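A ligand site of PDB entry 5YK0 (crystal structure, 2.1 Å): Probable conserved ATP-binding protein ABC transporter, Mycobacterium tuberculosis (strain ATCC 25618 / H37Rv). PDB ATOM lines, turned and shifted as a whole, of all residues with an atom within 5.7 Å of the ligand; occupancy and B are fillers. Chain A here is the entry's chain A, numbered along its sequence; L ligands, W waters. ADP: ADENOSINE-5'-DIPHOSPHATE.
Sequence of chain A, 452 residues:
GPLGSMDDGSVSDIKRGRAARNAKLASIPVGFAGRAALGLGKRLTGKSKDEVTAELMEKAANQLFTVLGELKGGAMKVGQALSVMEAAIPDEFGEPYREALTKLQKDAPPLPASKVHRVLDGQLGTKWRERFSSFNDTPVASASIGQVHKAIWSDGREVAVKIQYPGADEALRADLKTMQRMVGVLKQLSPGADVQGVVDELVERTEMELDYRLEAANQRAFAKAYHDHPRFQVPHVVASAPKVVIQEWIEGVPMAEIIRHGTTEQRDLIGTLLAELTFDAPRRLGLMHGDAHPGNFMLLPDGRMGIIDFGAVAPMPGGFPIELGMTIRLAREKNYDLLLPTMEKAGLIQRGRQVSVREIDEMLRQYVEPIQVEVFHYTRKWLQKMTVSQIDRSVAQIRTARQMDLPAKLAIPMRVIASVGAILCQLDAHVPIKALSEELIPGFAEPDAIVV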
ATOM      1  N   ALA A 141      13.300 -10.900  -1.186  1.00  0.00           N
ATOM      2  CA  ALA A 141      11.848 -10.780  -1.165  1.00  0.00           C
ATOM      3  C   ALA A 141      11.176 -12.137  -1.059  1.00  0.00           C
ATOM      4  O   ALA A 141      11.804 -13.187  -1.260  1.00  0.00           O
ATOM      5  CB  ALA A 141      11.356 -10.048  -2.401  1.00  0.00           C
ATOM      6  N   SER A 142       9.893 -12.132  -0.739  1.00  0.00           N
ATOM      7  CA  SER A 142       9.110 -13.358  -0.656  1.00  0.00           C
ATOM      8  C   SER A 142       8.143 -13.446  -1.825  1.00  0.00           C
ATOM      9  O   SER A 142       7.598 -12.443  -2.273  1.00  0.00           O
ATOM     10  CB  SER A 142       8.355 -13.429   0.672  1.00  0.00           C
ATOM     11  OG  SER A 142       9.249 -13.363   1.762  1.00  0.00           O
ATOM     12  N   ALA A 143       7.951 -14.670  -2.321  1.00  0.00           N
ATOM     13  CA  ALA A 143       6.940 -14.935  -3.338  1.00  0.00           C
ATOM     14  C   ALA A 143       5.830 -15.780  -2.717  1.00  0.00           C
ATOM     15  O   ALA A 143       5.953 -16.220  -1.581  1.00  0.00           O
ATOM     16  CB  ALA A 143       7.552 -15.634  -4.536  1.00  0.00           C
ATOM     17  N   SER A 144       4.758 -15.999  -3.476  1.00  0.00           N
ATOM     18  CA  SER A 144       3.595 -16.720  -2.960  1.00  0.00           C
ATOM     19  C   SER A 144       3.961 -18.109  -2.448  1.00  0.00           C
ATOM     20  O   SER A 144       3.590 -18.478  -1.339  1.00  0.00           O
ATOM     21  CB  SER A 144       2.514 -16.827  -4.038  1.00  0.00           C
ATOM     22  OG  SER A 144       2.944 -17.623  -5.116  1.00  0.00           O
ATOM     23  N   ILE A 145       4.703 -18.863  -3.246  1.00  0.00           N
ATOM     24  CA  ILE A 145       5.189 -20.173  -2.813  1.00  0.00           C
ATOM     25  C   ILE A 145       6.696 -20.322  -3.060  1.00  0.00           C
ATOM     26  O   ILE A 145       7.168 -21.384  -3.456  1.00  0.00           O
ATOM     27  CB  ILE A 145       4.442 -21.330  -3.507  1.00  0.00           C
ATOM     28  CG1 ILE A 145       4.531 -21.203  -5.035  1.00  0.00           C
ATOM     29  CG2 ILE A 145       2.983 -21.372  -3.065  1.00  0.00           C
ATOM     30  CD1 ILE A 145       4.065 -22.460  -5.766  1.00  0.00           C
ATOM     31  N   VAL A 148      12.688 -14.809  -3.534  1.00  0.00           N
ATOM     32  CA  VAL A 148      13.419 -14.182  -4.636  1.00  0.00           C
ATOM     33  C   VAL A 148      14.808 -13.756  -4.200  1.00  0.00           C
ATOM     34  O   VAL A 148      14.987 -13.146  -3.153  1.00  0.00           O
ATOM     35  CB  VAL A 148      12.646 -12.973  -5.194  1.00  0.00           C
ATOM     36  CG1 VAL A 148      13.397 -12.349  -6.361  1.00  0.00           C
ATOM     37  CG2 VAL A 148      11.248 -13.390  -5.618  1.00  0.00           C
ATOM     38  N   ALA A 160      16.647 -10.998 -11.010  1.00  0.00           N
ATOM     39  CA  ALA A 160      15.855 -11.599  -9.946  1.00  0.00           C
ATOM     40  C   ALA A 160      15.654 -13.079 -10.260  1.00  0.00           C
ATOM     41  O   ALA A 160      15.253 -13.446 -11.365  1.00  0.00           O
ATOM     42  CB  ALA A 160      14.519 -10.881  -9.804  1.00  0.00           C
ATOM     43  N   LYS A 162      13.583 -16.231  -8.916  1.00  0.00           N
ATOM     44  CA  LYS A 162      12.542 -16.782  -8.069  1.00  0.00           C
ATOM     45  C   LYS A 162      12.691 -18.288  -7.929  1.00  0.00           C
ATOM     46  O   LYS A 162      12.655 -19.049  -8.909  1.00  0.00           O
ATOM     47  CB  LYS A 162      11.146 -16.445  -8.617  1.00  0.00           C
ATOM     48  CG  LYS A 162      10.030 -16.899  -7.669  1.00  0.00           C
ATOM     49  CD  LYS A 162       8.721 -16.189  -7.949  1.00  0.00           C
ATOM     50  CE  LYS A 162       8.243 -16.390  -9.368  1.00  0.00           C
ATOM     51  NZ  LYS A 162       6.979 -15.657  -9.615  1.00  0.00           N
ATOM     52  N   GLU A 209       0.241 -21.835 -10.533  1.00  0.00           N
ATOM     53  CA  GLU A 209       1.060 -21.591  -9.349  1.00  0.00           C
ATOM     54  C   GLU A 209       2.350 -22.405  -9.355  1.00  0.00           C
ATOM     55  O   GLU A 209       3.394 -21.924  -8.924  1.00  0.00           O
ATOM     56  CB  GLU A 209       0.268 -21.874  -8.075  1.00  0.00           C
ATOM     57  CG  GLU A 209      -0.644 -20.750  -7.644  1.00  0.00           C
ATOM     58  CD  GLU A 209       0.122 -19.523  -7.194  1.00  0.00           C
ATOM     59  OE1 GLU A 209      -0.381 -18.402  -7.390  1.00  0.00           O
ATOM     60  OE2 GLU A 209       1.215 -19.682  -6.622  1.00  0.00           O
ATOM     61  N   TYR A 212       6.319 -22.415 -13.220  1.00  0.00           N
ATOM     62  CA  TYR A 212       6.748 -21.043 -13.474  1.00  0.00           C
ATOM     63  C   TYR A 212       6.891 -20.702 -14.959  1.00  0.00           C
ATOM     64  O   TYR A 212       6.877 -19.526 -15.355  1.00  0.00           O
ATOM     65  CB  TYR A 212       8.081 -20.783 -12.771  1.00  0.00           C
ATOM     66  CG  TYR A 212       7.988 -20.556 -11.266  1.00  0.00           C
ATOM     67  CD1 TYR A 212       6.770 -20.293 -10.649  1.00  0.00           C
ATOM     68  CD2 TYR A 212       9.128 -20.595 -10.471  1.00  0.00           C
ATOM     69  CE1 TYR A 212       6.694 -20.075  -9.279  1.00  0.00           C
ATOM     70  CE2 TYR A 212       9.060 -20.375  -9.113  1.00  0.00           C
ATOM     71  CZ  TYR A 212       7.849 -20.119  -8.519  1.00  0.00           C
ATOM     72  OH  TYR A 212       7.802 -19.898  -7.154  1.00  0.00           O
ATOM     73  N   GLU A 215       3.712 -18.445 -16.616  1.00  0.00           N
ATOM     74  CA  GLU A 215       3.841 -17.016 -16.393  1.00  0.00           C
ATOM     75  C   GLU A 215       5.068 -16.484 -17.134  1.00  0.00           C
ATOM     76  O   GLU A 215       5.025 -15.382 -17.680  1.00  0.00           O
ATOM     77  CB  GLU A 215       3.949 -16.687 -14.899  1.00  0.00           C
ATOM     78  CG  GLU A 215       4.067 -15.192 -14.641  1.00  0.00           C
ATOM     79  CD  GLU A 215       4.095 -14.829 -13.171  1.00  0.00           C
ATOM     80  OE1 GLU A 215       3.869 -15.737 -12.341  1.00  0.00           O
ATOM     81  OE2 GLU A 215       4.330 -13.647 -12.859  1.00  0.00           O
ATOM     82  N   GLN A 219       5.072 -13.385 -19.766  1.00  0.00           N
ATOM     83  CA  GLN A 219       6.010 -12.283 -19.578  1.00  0.00           C
ATOM     84  C   GLN A 219       6.881 -12.086 -20.810  1.00  0.00           C
ATOM     85  O   GLN A 219       7.210 -10.960 -21.149  1.00  0.00           O
ATOM     86  CB  GLN A 219       6.891 -12.500 -18.348  1.00  0.00           C
ATOM     87  CG  GLN A 219       7.864 -11.339 -18.102  1.00  0.00           C
ATOM     88  CD  GLN A 219       8.532 -11.375 -16.742  1.00  0.00           C
ATOM     89  OE1 GLN A 219       8.114 -12.107 -15.846  1.00  0.00           O
ATOM     90  NE2 GLN A 219       9.593 -10.581 -16.582  1.00  0.00           N
ATOM     91  N   PRO A 235      10.646  -6.441 -17.716  1.00  0.00           N
ATOM     92  CA  PRO A 235      11.947  -7.134 -17.698  1.00  0.00           C
ATOM     93  C   PRO A 235      11.915  -8.386 -18.571  1.00  0.00           C
ATOM     94  O   PRO A 235      10.919  -9.092 -18.596  1.00  0.00           O
ATOM     95  CB  PRO A 235      12.141  -7.490 -16.225  1.00  0.00           C
ATOM     96  CG  PRO A 235      10.790  -7.421 -15.614  1.00  0.00           C
ATOM     97  CD  PRO A 235      10.032  -6.388 -16.377  1.00  0.00           C
ATOM     98  N   GLN A 247      14.713 -13.378 -14.266  1.00  0.00           N
ATOM     99  CA  GLN A 247      14.404 -12.250 -15.138  1.00  0.00           C
ATOM    100  C   GLN A 247      15.264 -11.045 -14.809  1.00  0.00           C
ATOM    101  O   GLN A 247      15.846 -10.969 -13.742  1.00  0.00           O
ATOM    102  CB  GLN A 247      12.928 -11.877 -15.028  1.00  0.00           C
ATOM    103  CG  GLN A 247      12.482 -11.508 -13.633  1.00  0.00           C
ATOM    104  CD  GLN A 247      10.976 -11.328 -13.527  1.00  0.00           C
ATOM    105  OE1 GLN A 247      10.447 -10.247 -13.781  1.00  0.00           O
ATOM    106  NE2 GLN A 247      10.287 -12.393 -13.158  1.00  0.00           N
ATOM    107  N   GLU A 248      15.343 -10.094 -15.742  1.00  0.00           N
ATOM    108  CA  GLU A 248      16.107  -8.871 -15.536  1.00  0.00           C
ATOM    109  C   GLU A 248      15.654  -8.139 -14.284  1.00  0.00           C
ATOM    110  O   GLU A 248      14.462  -8.030 -14.016  1.00  0.00           O
ATOM    111  CB  GLU A 248      15.986  -7.951 -16.750  1.00  0.00           C
ATOM    112  CG  GLU A 248      16.591  -8.524 -18.022  1.00  0.00           C
ATOM    113  CD  GLU A 248      16.434  -7.600 -19.208  1.00  0.00           C
ATOM    114  OE1 GLU A 248      15.449  -6.833 -19.240  1.00  0.00           O
ATOM    115  OE2 GLU A 248      17.309  -7.618 -20.095  1.00  0.00           O
ATOM    116  N   TRP A 249      16.616  -7.651 -13.511  1.00  0.00           N
ATOM    117  CA  TRP A 249      16.304  -6.943 -12.286  1.00  0.00           C
ATOM    118  C   TRP A 249      15.862  -5.518 -12.569  1.00  0.00           C
ATOM    119  O   TRP A 249      16.561  -4.771 -13.261  1.00  0.00           O
ATOM    120  CB  TRP A 249      17.506  -6.935 -11.338  1.00  0.00           C
ATOM    121  CG  TRP A 249      17.245  -6.217 -10.051  1.00  0.00           C
ATOM    122  CD1 TRP A 249      17.397  -4.877  -9.817  1.00  0.00           C
ATOM    123  CD2 TRP A 249      16.774  -6.785  -8.832  1.00  0.00           C
ATOM    124  NE1 TRP A 249      17.055  -4.581  -8.516  1.00  0.00           N
ATOM    125  CE2 TRP A 249      16.667  -5.734  -7.892  1.00  0.00           C
ATOM    126  CE3 TRP A 249      16.424  -8.089  -8.436  1.00  0.00           C
ATOM    127  CZ2 TRP A 249      16.233  -5.952  -6.580  1.00  0.00           C
ATOM    128  CZ3 TRP A 249      15.997  -8.296  -7.135  1.00  0.00           C
ATOM    129  CH2 TRP A 249      15.903  -7.231  -6.228  1.00  0.00           C
ATOM    130  N   ILE A 250      14.705  -5.140 -12.049  1.00  0.00           N
ATOM    131  CA  ILE A 250      14.301  -3.748 -12.086  1.00  0.00           C
ATOM    132  C   ILE A 250      13.826  -3.331 -10.703  1.00  0.00           C
ATOM    133  O   ILE A 250      13.254  -4.127  -9.966  1.00  0.00           O
ATOM    134  CB  ILE A 250      13.164  -3.481 -13.114  1.00  0.00           C
ATOM    135  CG1 ILE A 250      11.899  -4.253 -12.745  1.00  0.00           C
ATOM    136  CG2 ILE A 250      13.628  -3.838 -14.522  1.00  0.00           C
ATOM    137  CD1 ILE A 250      10.691  -3.847 -13.569  1.00  0.00           C
ATOM    138  N   GLU A 251      14.096  -2.089 -10.333  1.00  0.00           N
ATOM    139  CA  GLU A 251      13.546  -1.589  -9.085  1.00  0.00           C
ATOM    140  C   GLU A 251      13.212  -0.115  -9.192  1.00  0.00           C
ATOM    141  O   GLU A 251      13.866   0.648  -9.896  1.00  0.00           O
ATOM    142  CB  GLU A 251      14.511  -1.843  -7.923  1.00  0.00           C
ATOM    143  CG  GLU A 251      15.833  -1.126  -8.010  1.00  0.00           C
ATOM    144  CD  GLU A 251      16.697  -1.384  -6.788  1.00  0.00           C
ATOM    145  OE1 GLU A 251      17.624  -2.218  -6.892  1.00  0.00           O
ATOM    146  OE2 GLU A 251      16.447  -0.769  -5.733  1.00  0.00           O
ATOM    147  N   GLY A 295       1.193  -4.957  -6.086  1.00  0.00           N
ATOM    148  CA  GLY A 295       2.451  -5.686  -6.042  1.00  0.00           C
ATOM    149  C   GLY A 295       3.035  -5.953  -7.406  1.00  0.00           C
ATOM    150  O   GLY A 295       4.230  -6.223  -7.530  1.00  0.00           O
ATOM    151  N   ASN A 296       2.204  -5.874  -8.450  1.00  0.00           N
ATOM    152  CA  ASN A 296       2.652  -6.115  -9.808  1.00  0.00           C
ATOM    153  C   ASN A 296       3.437  -4.951 -10.434  1.00  0.00           C
ATOM    154  O   ASN A 296       4.116  -5.142 -11.446  1.00  0.00           O
ATOM    155  CB  ASN A 296       1.460  -6.426 -10.723  1.00  0.00           C
ATOM    156  CG  ASN A 296       0.591  -7.551 -10.201  1.00  0.00           C
ATOM    157  OD1 ASN A 296       1.027  -8.369  -9.387  1.00  0.00           O
ATOM    158  ND2 ASN A 296      -0.644  -7.605 -10.677  1.00  0.00           N
ATOM    159  N   MET A 298       5.567  -0.892 -10.408  1.00  0.00           N
ATOM    160  CA  MET A 298       6.414   0.085  -9.731  1.00  0.00           C
ATOM    161  C   MET A 298       6.638   1.317 -10.585  1.00  0.00           C
ATOM    162  O   MET A 298       6.424   1.299 -11.789  1.00  0.00           O
ATOM    163  CB  MET A 298       7.746  -0.551  -9.329  1.00  0.00           C
ATOM    164  CG  MET A 298       8.600  -1.014 -10.510  1.00  0.00           C
ATOM    165  SD  MET A 298      10.010  -2.005  -9.967  1.00  0.00           S
ATOM    166  CE  MET A 298       9.165  -3.421  -9.271  1.00  0.00           C
ATOM    167  N   ILE A 308       6.045  -6.527 -13.271  1.00  0.00           N
ATOM    168  CA  ILE A 308       6.801  -7.748 -12.985  1.00  0.00           C
ATOM    169  C   ILE A 308       5.984  -9.032 -12.848  1.00  0.00           C
ATOM    170  O   ILE A 308       6.541 -10.129 -12.906  1.00  0.00           O
ATOM    171  CB  ILE A 308       7.640  -7.601 -11.697  1.00  0.00           C
ATOM    172  CG1 ILE A 308       6.742  -7.274 -10.506  1.00  0.00           C
ATOM    173  CG2 ILE A 308       8.699  -6.531 -11.880  1.00  0.00           C
ATOM    174  CD1 ILE A 308       7.493  -7.199  -9.185  1.00  0.00           C
ATOM    175  N   ASP A 309       4.671  -8.918 -12.680  1.00  0.00           N
ATOM    176  CA  ASP A 309       3.842 -10.125 -12.496  1.00  0.00           C
ATOM    177  C   ASP A 309       2.933 -10.326 -13.702  1.00  0.00           C
ATOM    178  O   ASP A 309       2.203  -9.416 -14.100  1.00  0.00           O
ATOM    179  CB  ASP A 309       3.020 -10.030 -11.208  1.00  0.00           C
ATOM    180  CG  ASP A 309       2.482 -11.378 -10.749  1.00  0.00           C
ATOM    181  OD1 ASP A 309       2.076 -12.196 -11.602  1.00  0.00           O
ATOM    182  OD2 ASP A 309       2.465 -11.627  -9.527  1.00  0.00           O
HETATM  183  PB  ADP L   1       4.711 -14.239  -6.921  1.00  0.00           P
HETATM  184  O1B ADP L   1       4.285 -13.806  -5.536  1.00  0.00           O
HETATM  185  O2B ADP L   1       3.864 -13.684  -8.028  1.00  0.00           O
HETATM  186  O3B ADP L   1       5.022 -15.719  -7.055  1.00  0.00           O
HETATM  187  PA  ADP L   1       6.255 -12.002  -7.633  1.00  0.00           P
HETATM  188  O1A ADP L   1       5.101 -11.248  -7.023  1.00  0.00           O
HETATM  189  O2A ADP L   1       6.489 -12.014  -9.123  1.00  0.00           O
HETATM  190  O3A ADP L   1       6.146 -13.541  -7.131  1.00  0.00           O
HETATM  191  O5' ADP L   1       7.593 -11.524  -6.879  1.00  0.00           O
HETATM  192  C5' ADP L   1       7.527 -11.195  -5.496  1.00  0.00           C
HETATM  193  C4' ADP L   1       8.621 -10.199  -5.139  1.00  0.00           C
HETATM  194  O4' ADP L   1       9.812 -10.498  -5.874  1.00  0.00           O
HETATM  195  C3' ADP L   1       8.237  -8.782  -5.504  1.00  0.00           C
HETATM  196  O3' ADP L   1       7.727  -8.089  -4.365  1.00  0.00           O
HETATM  197  C2' ADP L   1       9.518  -8.142  -5.984  1.00  0.00           C
HETATM  198  O2' ADP L   1      10.053  -7.334  -4.932  1.00  0.00           O
HETATM  199  C1' ADP L   1      10.468  -9.292  -6.281  1.00  0.00           C
HETATM  200  N9  ADP L   1      10.688  -9.327  -7.749  1.00  0.00           N
HETATM  201  C8  ADP L   1      10.060 -10.126  -8.631  1.00  0.00           C
HETATM  202  N7  ADP L   1      10.491  -9.901  -9.901  1.00  0.00           N
HETATM  203  C5  ADP L   1      11.422  -8.932  -9.841  1.00  0.00           C
HETATM  204  C6  ADP L   1      12.290  -8.210 -10.801  1.00  0.00           C
HETATM  205  N6  ADP L   1      12.236  -8.475 -12.128  1.00  0.00           N
HETATM  206  N1  ADP L   1      13.116  -7.262 -10.315  1.00  0.00           N
HETATM  207  C2  ADP L   1      13.175  -6.975  -9.007  1.00  0.00           C
HETATM  208  N3  ADP L   1      12.421  -7.582  -8.074  1.00  0.00           N
HETATM  209  C4  ADP L   1      11.542  -8.556  -8.418  1.00  0.00           C
HETATM  210  O   HOH W   1       3.038  -9.049  -8.085  1.00  0.00           O
HETATM  211  O   HOH W   2       2.048 -14.834 -10.398  1.00  0.00           O
HETATM  212  O   HOH W   3       5.631 -18.441  -6.289  1.00  0.00           O
HETATM  213  O   HOH W   4       8.008  -4.833  -3.538  1.00  0.00           O
HETATM  214  O   HOH W   5       3.677 -17.144  -9.261  1.00  0.00           O
HETATM  215  O   HOH W   6      12.497  -6.363  -5.387  1.00  0.00           O
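Water W3 lies within hydrogen-bond range of the side-chain hydroxyl (OH) of Tyr 212, an oxygen (O3B) of the ligand, the side-chain hydroxyl (OG) of Ser 144 and the backbone NH (N) of Ile 145. Water W5 bridges O3B of the ligand (3.0 Å) and OE1 of Glu 215 (3.4 Å). Water W2 lies within hydrogen-bond range of OE1 of Glu 215, OD1 of Asp 309 and O2B of the ligand.
An oxygen (O2B) of the ligand sits close to the side-chain carboxylate (OD2) of Asp 309, 2.9 Å away. An oxygen (O3B) of the ligand lies within hydrogen-bond range of the side-chain hydroxyl (OG) of Ser 144 (3.4 Å). N6 of the ligand is in hydrogen-bond range of O of Glu 248. The side-chain amino group (NZ) of Lys 162 is in salt-bridge range of an oxygen (O3B) of the ligand (3.2 Å). The backbone NH (N) of Ser 144 lies within hydrogen-bond range of an oxygen (O1B) of the ligand (3.0 Å). A nitrogen (N6) of the ligand lies within hydrogen-bond range of the side-chain amide oxygen of Gln 247. The backbone NH (N) of Ile 250 lies within hydrogen-bond range of a nitrogen (N1) of the ligand.
N of Val 148 lies within hydrogen-bond range of O of Ala 141 (2.9 Å). The side-chain amide nitrogen of Gln 219 sits at hydrogen-bond distance from the side-chain amide oxygen of Gln 247. NE1 of Trp 249 lies within hydrogen-bond range of OE1 of Glu 251 (2.9 Å). The backbone carbonyl oxygen of Gln 247 is in hydrogen-bond range of the backbone NH of Ala 160. The side-chain amide nitrogen (NE2) of Gln 219 sits at hydrogen-bond distance from the backbone carbonyl oxygen (O) of Pro 235. The side-chain hydroxyl (OG) of Ser 144 lies within hydrogen-bond range of the side-chain carboxylate (OE2) of Glu 209, at 3.1 Å. The backbone carbonyl oxygen of Asn 296 is in hydrogen-bond range of the backbone NH of Ile 308 (3.0 Å).
Residues that only touch the ligand: Val 148, Ser 142, Trp 249, Ala 143, Ala 160, Ala 141, Ile 308 and Pro 235.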
